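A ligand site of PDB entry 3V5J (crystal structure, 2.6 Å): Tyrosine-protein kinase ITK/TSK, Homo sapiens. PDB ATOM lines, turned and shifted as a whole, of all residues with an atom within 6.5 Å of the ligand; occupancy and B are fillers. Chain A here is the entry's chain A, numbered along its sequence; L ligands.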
ATOM      1  N   ILE A  15     -18.045 -19.594  24.315  1.00  0.00           N
ATOM      2  CA  ILE A  15     -18.700 -20.631  25.125  1.00  0.00           C
ATOM      3  C   ILE A  15     -17.876 -21.916  25.303  1.00  0.00           C
ATOM      4  O   ILE A  15     -18.001 -22.584  26.330  1.00  0.00           O
ATOM      5  CB  ILE A  15     -20.184 -20.885  24.691  1.00  0.00           C
ATOM      6  CG1 ILE A  15     -20.277 -21.328  23.198  1.00  0.00           C
ATOM      7  CG2 ILE A  15     -21.067 -19.663  24.998  1.00  0.00           C
ATOM      8  CD1 ILE A  15     -21.697 -21.605  22.640  1.00  0.00           C
ATOM      9  N   GLY A  16     -17.041 -22.235  24.306  1.00  0.00           N
ATOM     10  CA  GLY A  16     -16.185 -23.412  24.316  1.00  0.00           C
ATOM     11  C   GLY A  16     -14.744 -23.144  23.924  1.00  0.00           C
ATOM     12  O   GLY A  16     -14.462 -22.150  23.243  1.00  0.00           O
ATOM     13  N   SER A  17     -13.827 -24.025  24.362  1.00  0.00           N
ATOM     14  CA  SER A  17     -12.394 -23.939  24.100  1.00  0.00           C
ATOM     15  C   SER A  17     -11.747 -25.327  23.935  1.00  0.00           C
ATOM     16  O   SER A  17     -12.397 -26.341  24.185  1.00  0.00           O
ATOM     17  CB  SER A  17     -11.693 -23.132  25.196  1.00  0.00           C
ATOM     18  N   GLN A  19     -10.031 -28.352  21.692  1.00  0.00           N
ATOM     19  CA  GLN A  19     -10.145 -29.084  20.416  1.00  0.00           C
ATOM     20  C   GLN A  19      -9.161 -28.669  19.322  1.00  0.00           C
ATOM     21  O   GLN A  19      -7.967 -28.525  19.570  1.00  0.00           O
ATOM     22  CB  GLN A  19     -11.587 -29.058  19.894  1.00  0.00           C
ATOM     23  N   GLY A  21     -12.022 -26.340  17.589  1.00  0.00           N
ATOM     24  CA  GLY A  21     -11.207 -25.346  18.286  1.00  0.00           C
ATOM     25  C   GLY A  21     -11.975 -24.560  19.321  1.00  0.00           C
ATOM     26  O   GLY A  21     -12.086 -24.991  20.469  1.00  0.00           O
ATOM     27  N   VAL A  23     -15.658 -22.480  20.367  1.00  0.00           N
ATOM     28  CA  VAL A  23     -17.104 -22.404  20.149  1.00  0.00           C
ATOM     29  C   VAL A  23     -17.590 -21.057  20.686  1.00  0.00           C
ATOM     30  O   VAL A  23     -17.306 -20.698  21.833  1.00  0.00           O
ATOM     31  CB  VAL A  23     -17.888 -23.611  20.748  1.00  0.00           C
ATOM     32  CG1 VAL A  23     -19.347 -23.592  20.310  1.00  0.00           C
ATOM     33  CG2 VAL A  23     -17.242 -24.944  20.373  1.00  0.00           C
ATOM     34  N   LEU A  25     -21.000 -18.147  20.849  1.00  0.00           N
ATOM     35  CA  LEU A  25     -22.431 -17.859  20.746  1.00  0.00           C
ATOM     36  C   LEU A  25     -22.513 -16.572  19.927  1.00  0.00           C
ATOM     37  O   LEU A  25     -21.787 -15.617  20.209  1.00  0.00           O
ATOM     38  CB  LEU A  25     -23.066 -17.670  22.141  1.00  0.00           C
ATOM     39  CG  LEU A  25     -24.406 -16.894  22.222  1.00  0.00           C
ATOM     40  CD1 LEU A  25     -25.564 -17.692  21.647  1.00  0.00           C
ATOM     41  CD2 LEU A  25     -24.707 -16.499  23.652  1.00  0.00           C
ATOM     42  N   VAL A  34     -26.856 -18.502  16.687  1.00  0.00           N
ATOM     43  CA  VAL A  34     -25.980 -19.500  16.082  1.00  0.00           C
ATOM     44  C   VAL A  34     -24.782 -19.882  16.943  1.00  0.00           C
ATOM     45  O   VAL A  34     -24.326 -19.075  17.766  1.00  0.00           O
ATOM     46  CB  VAL A  34     -25.550 -19.130  14.627  1.00  0.00           C
ATOM     47  CG1 VAL A  34     -26.728 -19.157  13.668  1.00  0.00           C
ATOM     48  CG2 VAL A  34     -24.824 -17.789  14.574  1.00  0.00           C
ATOM     49  N   ALA A  35     -24.257 -21.102  16.747  1.00  0.00           N
ATOM     50  CA  ALA A  35     -23.062 -21.595  17.417  1.00  0.00           C
ATOM     51  C   ALA A  35     -21.946 -21.610  16.379  1.00  0.00           C
ATOM     52  O   ALA A  35     -22.005 -22.370  15.413  1.00  0.00           O
ATOM     53  CB  ALA A  35     -23.299 -22.987  17.974  1.00  0.00           C
ATOM     54  N   LYS A  37     -18.274 -22.394  15.311  1.00  0.00           N
ATOM     55  CA  LYS A  37     -17.144 -23.274  15.618  1.00  0.00           C
ATOM     56  C   LYS A  37     -15.921 -22.866  14.786  1.00  0.00           C
ATOM     57  O   LYS A  37     -15.824 -23.221  13.611  1.00  0.00           O
ATOM     58  CB  LYS A  37     -17.518 -24.752  15.427  1.00  0.00           C
ATOM     59  CG  LYS A  37     -16.587 -25.724  16.144  1.00  0.00           C
ATOM     60  CD  LYS A  37     -16.990 -27.172  15.914  1.00  0.00           C
ATOM     61  CE  LYS A  37     -16.069 -28.124  16.633  1.00  0.00           C
ATOM     62  NZ  LYS A  37     -16.425 -29.533  16.366  1.00  0.00           N
ATOM     63  N   VAL A  65     -27.521 -32.607  14.590  1.00  0.00           N
ATOM     64  CA  VAL A  65     -27.323 -31.162  14.529  1.00  0.00           C
ATOM     65  C   VAL A  65     -27.299 -30.644  13.078  1.00  0.00           C
ATOM     66  O   VAL A  65     -26.801 -31.338  12.174  1.00  0.00           O
ATOM     67  CB  VAL A  65     -26.121 -30.686  15.406  1.00  0.00           C
ATOM     68  CG1 VAL A  65     -24.777 -30.944  14.740  1.00  0.00           C
ATOM     69  CG2 VAL A  65     -26.272 -29.219  15.816  1.00  0.00           C
ATOM     70  N   PHE A  81     -23.362 -23.344  12.990  1.00  0.00           N
ATOM     71  CA  PHE A  81     -24.305 -24.362  13.475  1.00  0.00           C
ATOM     72  C   PHE A  81     -25.546 -23.720  14.104  1.00  0.00           C
ATOM     73  O   PHE A  81     -25.508 -22.540  14.467  1.00  0.00           O
ATOM     74  CB  PHE A  81     -23.635 -25.229  14.551  1.00  0.00           C
ATOM     75  CG  PHE A  81     -22.601 -26.221  14.088  1.00  0.00           C
ATOM     76  CD1 PHE A  81     -21.262 -25.878  14.023  1.00  0.00           C
ATOM     77  CD2 PHE A  81     -22.959 -27.541  13.788  1.00  0.00           C
ATOM     78  CE1 PHE A  81     -20.296 -26.813  13.630  1.00  0.00           C
ATOM     79  CE2 PHE A  81     -21.997 -28.467  13.392  1.00  0.00           C
ATOM     80  CZ  PHE A  81     -20.668 -28.098  13.316  1.00  0.00           C
ATOM     81  N   GLU A  82     -26.619 -24.517  14.291  1.00  0.00           N
ATOM     82  CA  GLU A  82     -27.833 -24.078  14.991  1.00  0.00           C
ATOM     83  C   GLU A  82     -27.495 -24.062  16.493  1.00  0.00           C
ATOM     84  O   GLU A  82     -26.784 -24.957  16.959  1.00  0.00           O
ATOM     85  CB  GLU A  82     -29.041 -24.989  14.678  1.00  0.00           C
ATOM     86  CG  GLU A  82     -28.895 -26.449  15.105  1.00  0.00           C
ATOM     87  CD  GLU A  82     -30.130 -27.325  15.024  1.00  0.00           C
ATOM     88  OE1 GLU A  82     -31.263 -26.786  15.020  1.00  0.00           O
ATOM     89  OE2 GLU A  82     -29.968 -28.563  15.009  1.00  0.00           O
ATOM     90  N   PHE A  83     -27.937 -23.034  17.224  1.00  0.00           N
ATOM     91  CA  PHE A  83     -27.626 -22.953  18.656  1.00  0.00           C
ATOM     92  C   PHE A  83     -28.463 -23.897  19.509  1.00  0.00           C
ATOM     93  O   PHE A  83     -29.692 -23.887  19.428  1.00  0.00           O
ATOM     94  CB  PHE A  83     -27.681 -21.505  19.181  1.00  0.00           C
ATOM     95  CG  PHE A  83     -27.212 -21.351  20.608  1.00  0.00           C
ATOM     96  CD1 PHE A  83     -25.852 -21.412  20.923  1.00  0.00           C
ATOM     97  CD2 PHE A  83     -28.118 -21.161  21.644  1.00  0.00           C
ATOM     98  CE1 PHE A  83     -25.422 -21.291  22.246  1.00  0.00           C
ATOM     99  CE2 PHE A  83     -27.688 -21.040  22.967  1.00  0.00           C
ATOM    100  CZ  PHE A  83     -26.338 -21.092  23.255  1.00  0.00           C
ATOM    101  N   MET A  84     -27.780 -24.730  20.310  1.00  0.00           N
ATOM    102  CA  MET A  84     -28.391 -25.681  21.234  1.00  0.00           C
ATOM    103  C   MET A  84     -28.327 -25.039  22.624  1.00  0.00           C
ATOM    104  O   MET A  84     -27.231 -24.833  23.160  1.00  0.00           O
ATOM    105  CB  MET A  84     -27.689 -27.048  21.182  1.00  0.00           C
ATOM    106  CG  MET A  84     -27.784 -27.736  19.825  1.00  0.00           C
ATOM    107  SD  MET A  84     -29.447 -28.303  19.362  1.00  0.00           S
ATOM    108  CE  MET A  84     -29.559 -29.795  20.327  1.00  0.00           C
ATOM    109  N   GLU A  85     -29.501 -24.671  23.160  1.00  0.00           N
ATOM    110  CA  GLU A  85     -29.693 -23.962  24.431  1.00  0.00           C
ATOM    111  C   GLU A  85     -28.991 -24.511  25.669  1.00  0.00           C
ATOM    112  O   GLU A  85     -28.500 -23.719  26.476  1.00  0.00           O
ATOM    113  CB  GLU A  85     -31.187 -23.752  24.718  1.00  0.00           C
ATOM    114  CG  GLU A  85     -31.887 -22.757  23.794  1.00  0.00           C
ATOM    115  CD  GLU A  85     -31.558 -21.290  24.004  1.00  0.00           C
ATOM    116  OE1 GLU A  85     -31.555 -20.837  25.179  1.00  0.00           O
ATOM    117  OE2 GLU A  85     -31.342 -20.587  23.000  1.00  0.00           O
ATOM    118  N   HIS A  86     -28.952 -25.840  25.840  1.00  0.00           N
ATOM    119  CA  HIS A  86     -28.379 -26.457  27.038  1.00  0.00           C
ATOM    120  C   HIS A  86     -26.962 -27.065  26.954  1.00  0.00           C
ATOM    121  O   HIS A  86     -26.548 -27.778  27.868  1.00  0.00           O
ATOM    122  CB  HIS A  86     -29.407 -27.389  27.710  1.00  0.00           C
ATOM    123  CG  HIS A  86     -30.632 -26.673  28.163  1.00  0.00           C
ATOM    124  ND1 HIS A  86     -30.671 -25.986  29.363  1.00  0.00           N
ATOM    125  CD2 HIS A  86     -31.822 -26.513  27.546  1.00  0.00           C
ATOM    126  CE1 HIS A  86     -31.877 -25.455  29.444  1.00  0.00           C
ATOM    127  NE2 HIS A  86     -32.611 -25.749  28.372  1.00  0.00           N
ATOM    128  N   GLY A  87     -26.233 -26.727  25.897  1.00  0.00           N
ATOM    129  CA  GLY A  87     -24.850 -27.160  25.681  1.00  0.00           C
ATOM    130  C   GLY A  87     -24.664 -28.652  25.464  1.00  0.00           C
ATOM    131  O   GLY A  87     -25.607 -29.361  25.098  1.00  0.00           O
ATOM    132  N   CYS A  88     -23.420 -29.128  25.689  1.00  0.00           N
ATOM    133  CA  CYS A  88     -23.097 -30.547  25.515  1.00  0.00           C
ATOM    134  C   CYS A  88     -23.650 -31.431  26.639  1.00  0.00           C
ATOM    135  O   CYS A  88     -23.737 -30.991  27.786  1.00  0.00           O
ATOM    136  CB  CYS A  88     -21.600 -30.767  25.286  1.00  0.00           C
ATOM    137  SG  CYS A  88     -20.583 -30.688  26.775  1.00  0.00           S
ATOM    138  N   ASP A  91     -21.650 -32.046  30.081  1.00  0.00           N
ATOM    139  CA  ASP A  91     -21.728 -30.934  31.030  1.00  0.00           C
ATOM    140  C   ASP A  91     -23.124 -30.804  31.655  1.00  0.00           C
ATOM    141  O   ASP A  91     -23.229 -30.506  32.842  1.00  0.00           O
ATOM    142  CB  ASP A  91     -21.298 -29.613  30.385  1.00  0.00           C
ATOM    143  CG  ASP A  91     -19.810 -29.484  30.088  1.00  0.00           C
ATOM    144  OD1 ASP A  91     -19.455 -28.662  29.214  1.00  0.00           O
ATOM    145  OD2 ASP A  91     -19.007 -30.172  30.753  1.00  0.00           O
ATOM    146  N   ARG A 132     -19.753 -35.765  25.217  1.00  0.00           N
ATOM    147  CA  ARG A 132     -19.163 -34.459  24.895  1.00  0.00           C
ATOM    148  C   ARG A 132     -19.477 -34.042  23.447  1.00  0.00           C
ATOM    149  O   ARG A 132     -19.454 -32.843  23.145  1.00  0.00           O
ATOM    150  CB  ARG A 132     -17.644 -34.458  25.175  1.00  0.00           C
ATOM    151  CG  ARG A 132     -16.818 -35.369  24.258  1.00  0.00           C
ATOM    152  CD  ARG A 132     -15.339 -35.302  24.572  1.00  0.00           C
ATOM    153  NE  ARG A 132     -14.539 -35.976  23.554  1.00  0.00           N
ATOM    154  CZ  ARG A 132     -14.247 -37.274  23.545  1.00  0.00           C
ATOM    155  NH1 ARG A 132     -14.699 -38.061  24.518  1.00  0.00           N
ATOM    156  NH2 ARG A 132     -13.502 -37.790  22.577  1.00  0.00           N
ATOM    157  N   LEU A 135     -25.400 -32.867  21.988  1.00  0.00           N
ATOM    158  CA  LEU A 135     -25.924 -31.579  22.473  1.00  0.00           C
ATOM    159  C   LEU A 135     -27.364 -31.645  22.968  1.00  0.00           C
ATOM    160  O   LEU A 135     -28.154 -32.437  22.468  1.00  0.00           O
ATOM    161  CB  LEU A 135     -25.770 -30.490  21.405  1.00  0.00           C
ATOM    162  CG  LEU A 135     -24.344 -30.091  21.041  1.00  0.00           C
ATOM    163  CD1 LEU A 135     -24.248 -29.739  19.591  1.00  0.00           C
ATOM    164  CD2 LEU A 135     -23.848 -28.950  21.915  1.00  0.00           C
ATOM    165  N   VAL A 136     -27.688 -30.789  23.958  1.00  0.00           N
ATOM    166  CA  VAL A 136     -29.019 -30.695  24.572  1.00  0.00           C
ATOM    167  C   VAL A 136     -29.703 -29.414  24.096  1.00  0.00           C
ATOM    168  O   VAL A 136     -29.117 -28.328  24.209  1.00  0.00           O
ATOM    169  CB  VAL A 136     -28.963 -30.783  26.130  1.00  0.00           C
ATOM    170  CG1 VAL A 136     -30.342 -31.016  26.721  1.00  0.00           C
ATOM    171  CG2 VAL A 136     -27.978 -31.840  26.603  1.00  0.00           C
ATOM    172  N   SER A 145     -23.609 -34.580  17.372  1.00  0.00           N
ATOM    173  CA  SER A 145     -22.777 -33.604  16.663  1.00  0.00           C
ATOM    174  C   SER A 145     -21.446 -34.216  16.221  1.00  0.00           C
ATOM    175  O   SER A 145     -21.024 -35.231  16.767  1.00  0.00           O
ATOM    176  CB  SER A 145     -22.540 -32.374  17.531  1.00  0.00           C
ATOM    177  OG  SER A 145     -21.972 -31.310  16.792  1.00  0.00           O
ATOM    178  N   ASP A 146     -20.783 -33.569  15.228  1.00  0.00           N
ATOM    179  CA  ASP A 146     -19.491 -33.960  14.630  1.00  0.00           C
ATOM    180  C   ASP A 146     -19.501 -35.395  14.057  1.00  0.00           C
ATOM    181  O   ASP A 146     -18.754 -36.266  14.519  1.00  0.00           O
ATOM    182  CB  ASP A 146     -18.310 -33.719  15.603  1.00  0.00           C
ATOM    183  CG  ASP A 146     -18.241 -32.314  16.182  1.00  0.00           C
ATOM    184  OD1 ASP A 146     -18.055 -32.189  17.417  1.00  0.00           O
ATOM    185  OD2 ASP A 146     -18.362 -31.338  15.405  1.00  0.00           O
HETATM  186  C1  LIG L   1     -16.804 -27.452  25.103  1.00  0.00           C
HETATM  187  C2  LIG L   1     -16.388 -28.686  24.283  1.00  0.00           C
HETATM  188  O1  LIG L   1     -16.637 -28.444  22.879  1.00  0.00           O
HETATM  189  C3  LIG L   1     -18.030 -28.157  22.616  1.00  0.00           C
HETATM  190  C4  LIG L   1     -18.449 -26.902  23.408  1.00  0.00           C
HETATM  191  N1  LIG L   1     -18.213 -27.135  24.848  1.00  0.00           N
HETATM  192  C5  LIG L   1     -18.603 -25.932  25.620  1.00  0.00           C
HETATM  193  C6  LIG L   1     -20.124 -25.812  25.679  1.00  0.00           C
HETATM  194  O2  LIG L   1     -20.541 -24.854  24.692  1.00  0.00           O
HETATM  195  C7  LIG L   1     -21.868 -24.558  24.766  1.00  0.00           C
HETATM  196  C8  LIG L   1     -22.419 -23.992  25.922  1.00  0.00           C
HETATM  197  C9  LIG L   1     -23.768 -23.644  25.976  1.00  0.00           C
HETATM  198  C10 LIG L   1     -24.378 -23.063  27.260  1.00  0.00           C
HETATM  199  C11 LIG L   1     -25.295 -24.123  27.873  1.00  0.00           C
HETATM  200  C12 LIG L   1     -25.866 -23.697  29.221  1.00  0.00           C
HETATM  201  C13 LIG L   1     -25.202 -21.809  26.948  1.00  0.00           C
HETATM  202  C14 LIG L   1     -24.318 -20.662  26.443  1.00  0.00           C
HETATM  203  O3  LIG L   1     -23.349 -22.733  28.210  1.00  0.00           O
HETATM  204  C15 LIG L   1     -24.575 -23.853  24.845  1.00  0.00           C
HETATM  205  C16 LIG L   1     -24.019 -24.405  23.687  1.00  0.00           C
HETATM  206  N2  LIG L   1     -24.548 -24.716  22.507  1.00  0.00           N
HETATM  207  C17 LIG L   1     -22.679 -24.764  23.644  1.00  0.00           C
HETATM  208  C18 LIG L   1     -22.445 -25.240  22.429  1.00  0.00           C
HETATM  209  C19 LIG L   1     -23.588 -25.229  21.734  1.00  0.00           C
HETATM  210  C20 LIG L   1     -23.775 -25.661  20.423  1.00  0.00           C
HETATM  211  C21 LIG L   1     -22.828 -26.314  19.658  1.00  0.00           C
HETATM  212  S1  LIG L   1     -21.262 -26.932  19.542  1.00  0.00           S
HETATM  213  C22 LIG L   1     -21.411 -27.499  17.962  1.00  0.00           C
HETATM  214  C23 LIG L   1     -22.648 -27.199  17.544  1.00  0.00           C
HETATM  215  C24 LIG L   1     -23.444 -26.563  18.432  1.00  0.00           C
HETATM  216  N3  LIG L   1     -24.688 -26.073  18.563  1.00  0.00           N
HETATM  217  N4  LIG L   1     -24.874 -25.575  19.671  1.00  0.00           N
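The backbone NH (N) of Met 84 is in hydrogen-bond range of a nitrogen (N4) of the ligand (3.1 Å).
O of Met 84 sits at hydrogen-bond distance from N2 of the ligand.
O of Glu 82 is in hydrogen-bond range of N3 of the ligand (2.9 Å).
Merely in contact with the ligand: Gly 87 (3.4 Å), Ala 35 (3.4 Å), Ile 15 (3.5 Å), Leu 135 (3.5 Å), His 86 (3.5 Å), Glu 85 (3.5 Å), Phe 83 (3.5 Å), Phe 81 (3.6 Å), Gly 16 (3.7 Å) and Val 23 (3.8 Å).
N of Val 136 is in hydrogen-bond range of O of Gly 87 (2.8 Å).
The backbone carbonyl oxygen (O) of Ala 35 is in hydrogen-bond range of the backbone NH (N) of Phe 81.
N of Ile 15 lies within hydrogen-bond range of O of Val 23 (2.8 Å).
The backbone NH (N) of His 86 sits at hydrogen-bond distance from the backbone carbonyl oxygen (O) of Val 136.
N of Gly 16 lies within hydrogen-bond range of O of Val 23 (2.9 Å).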
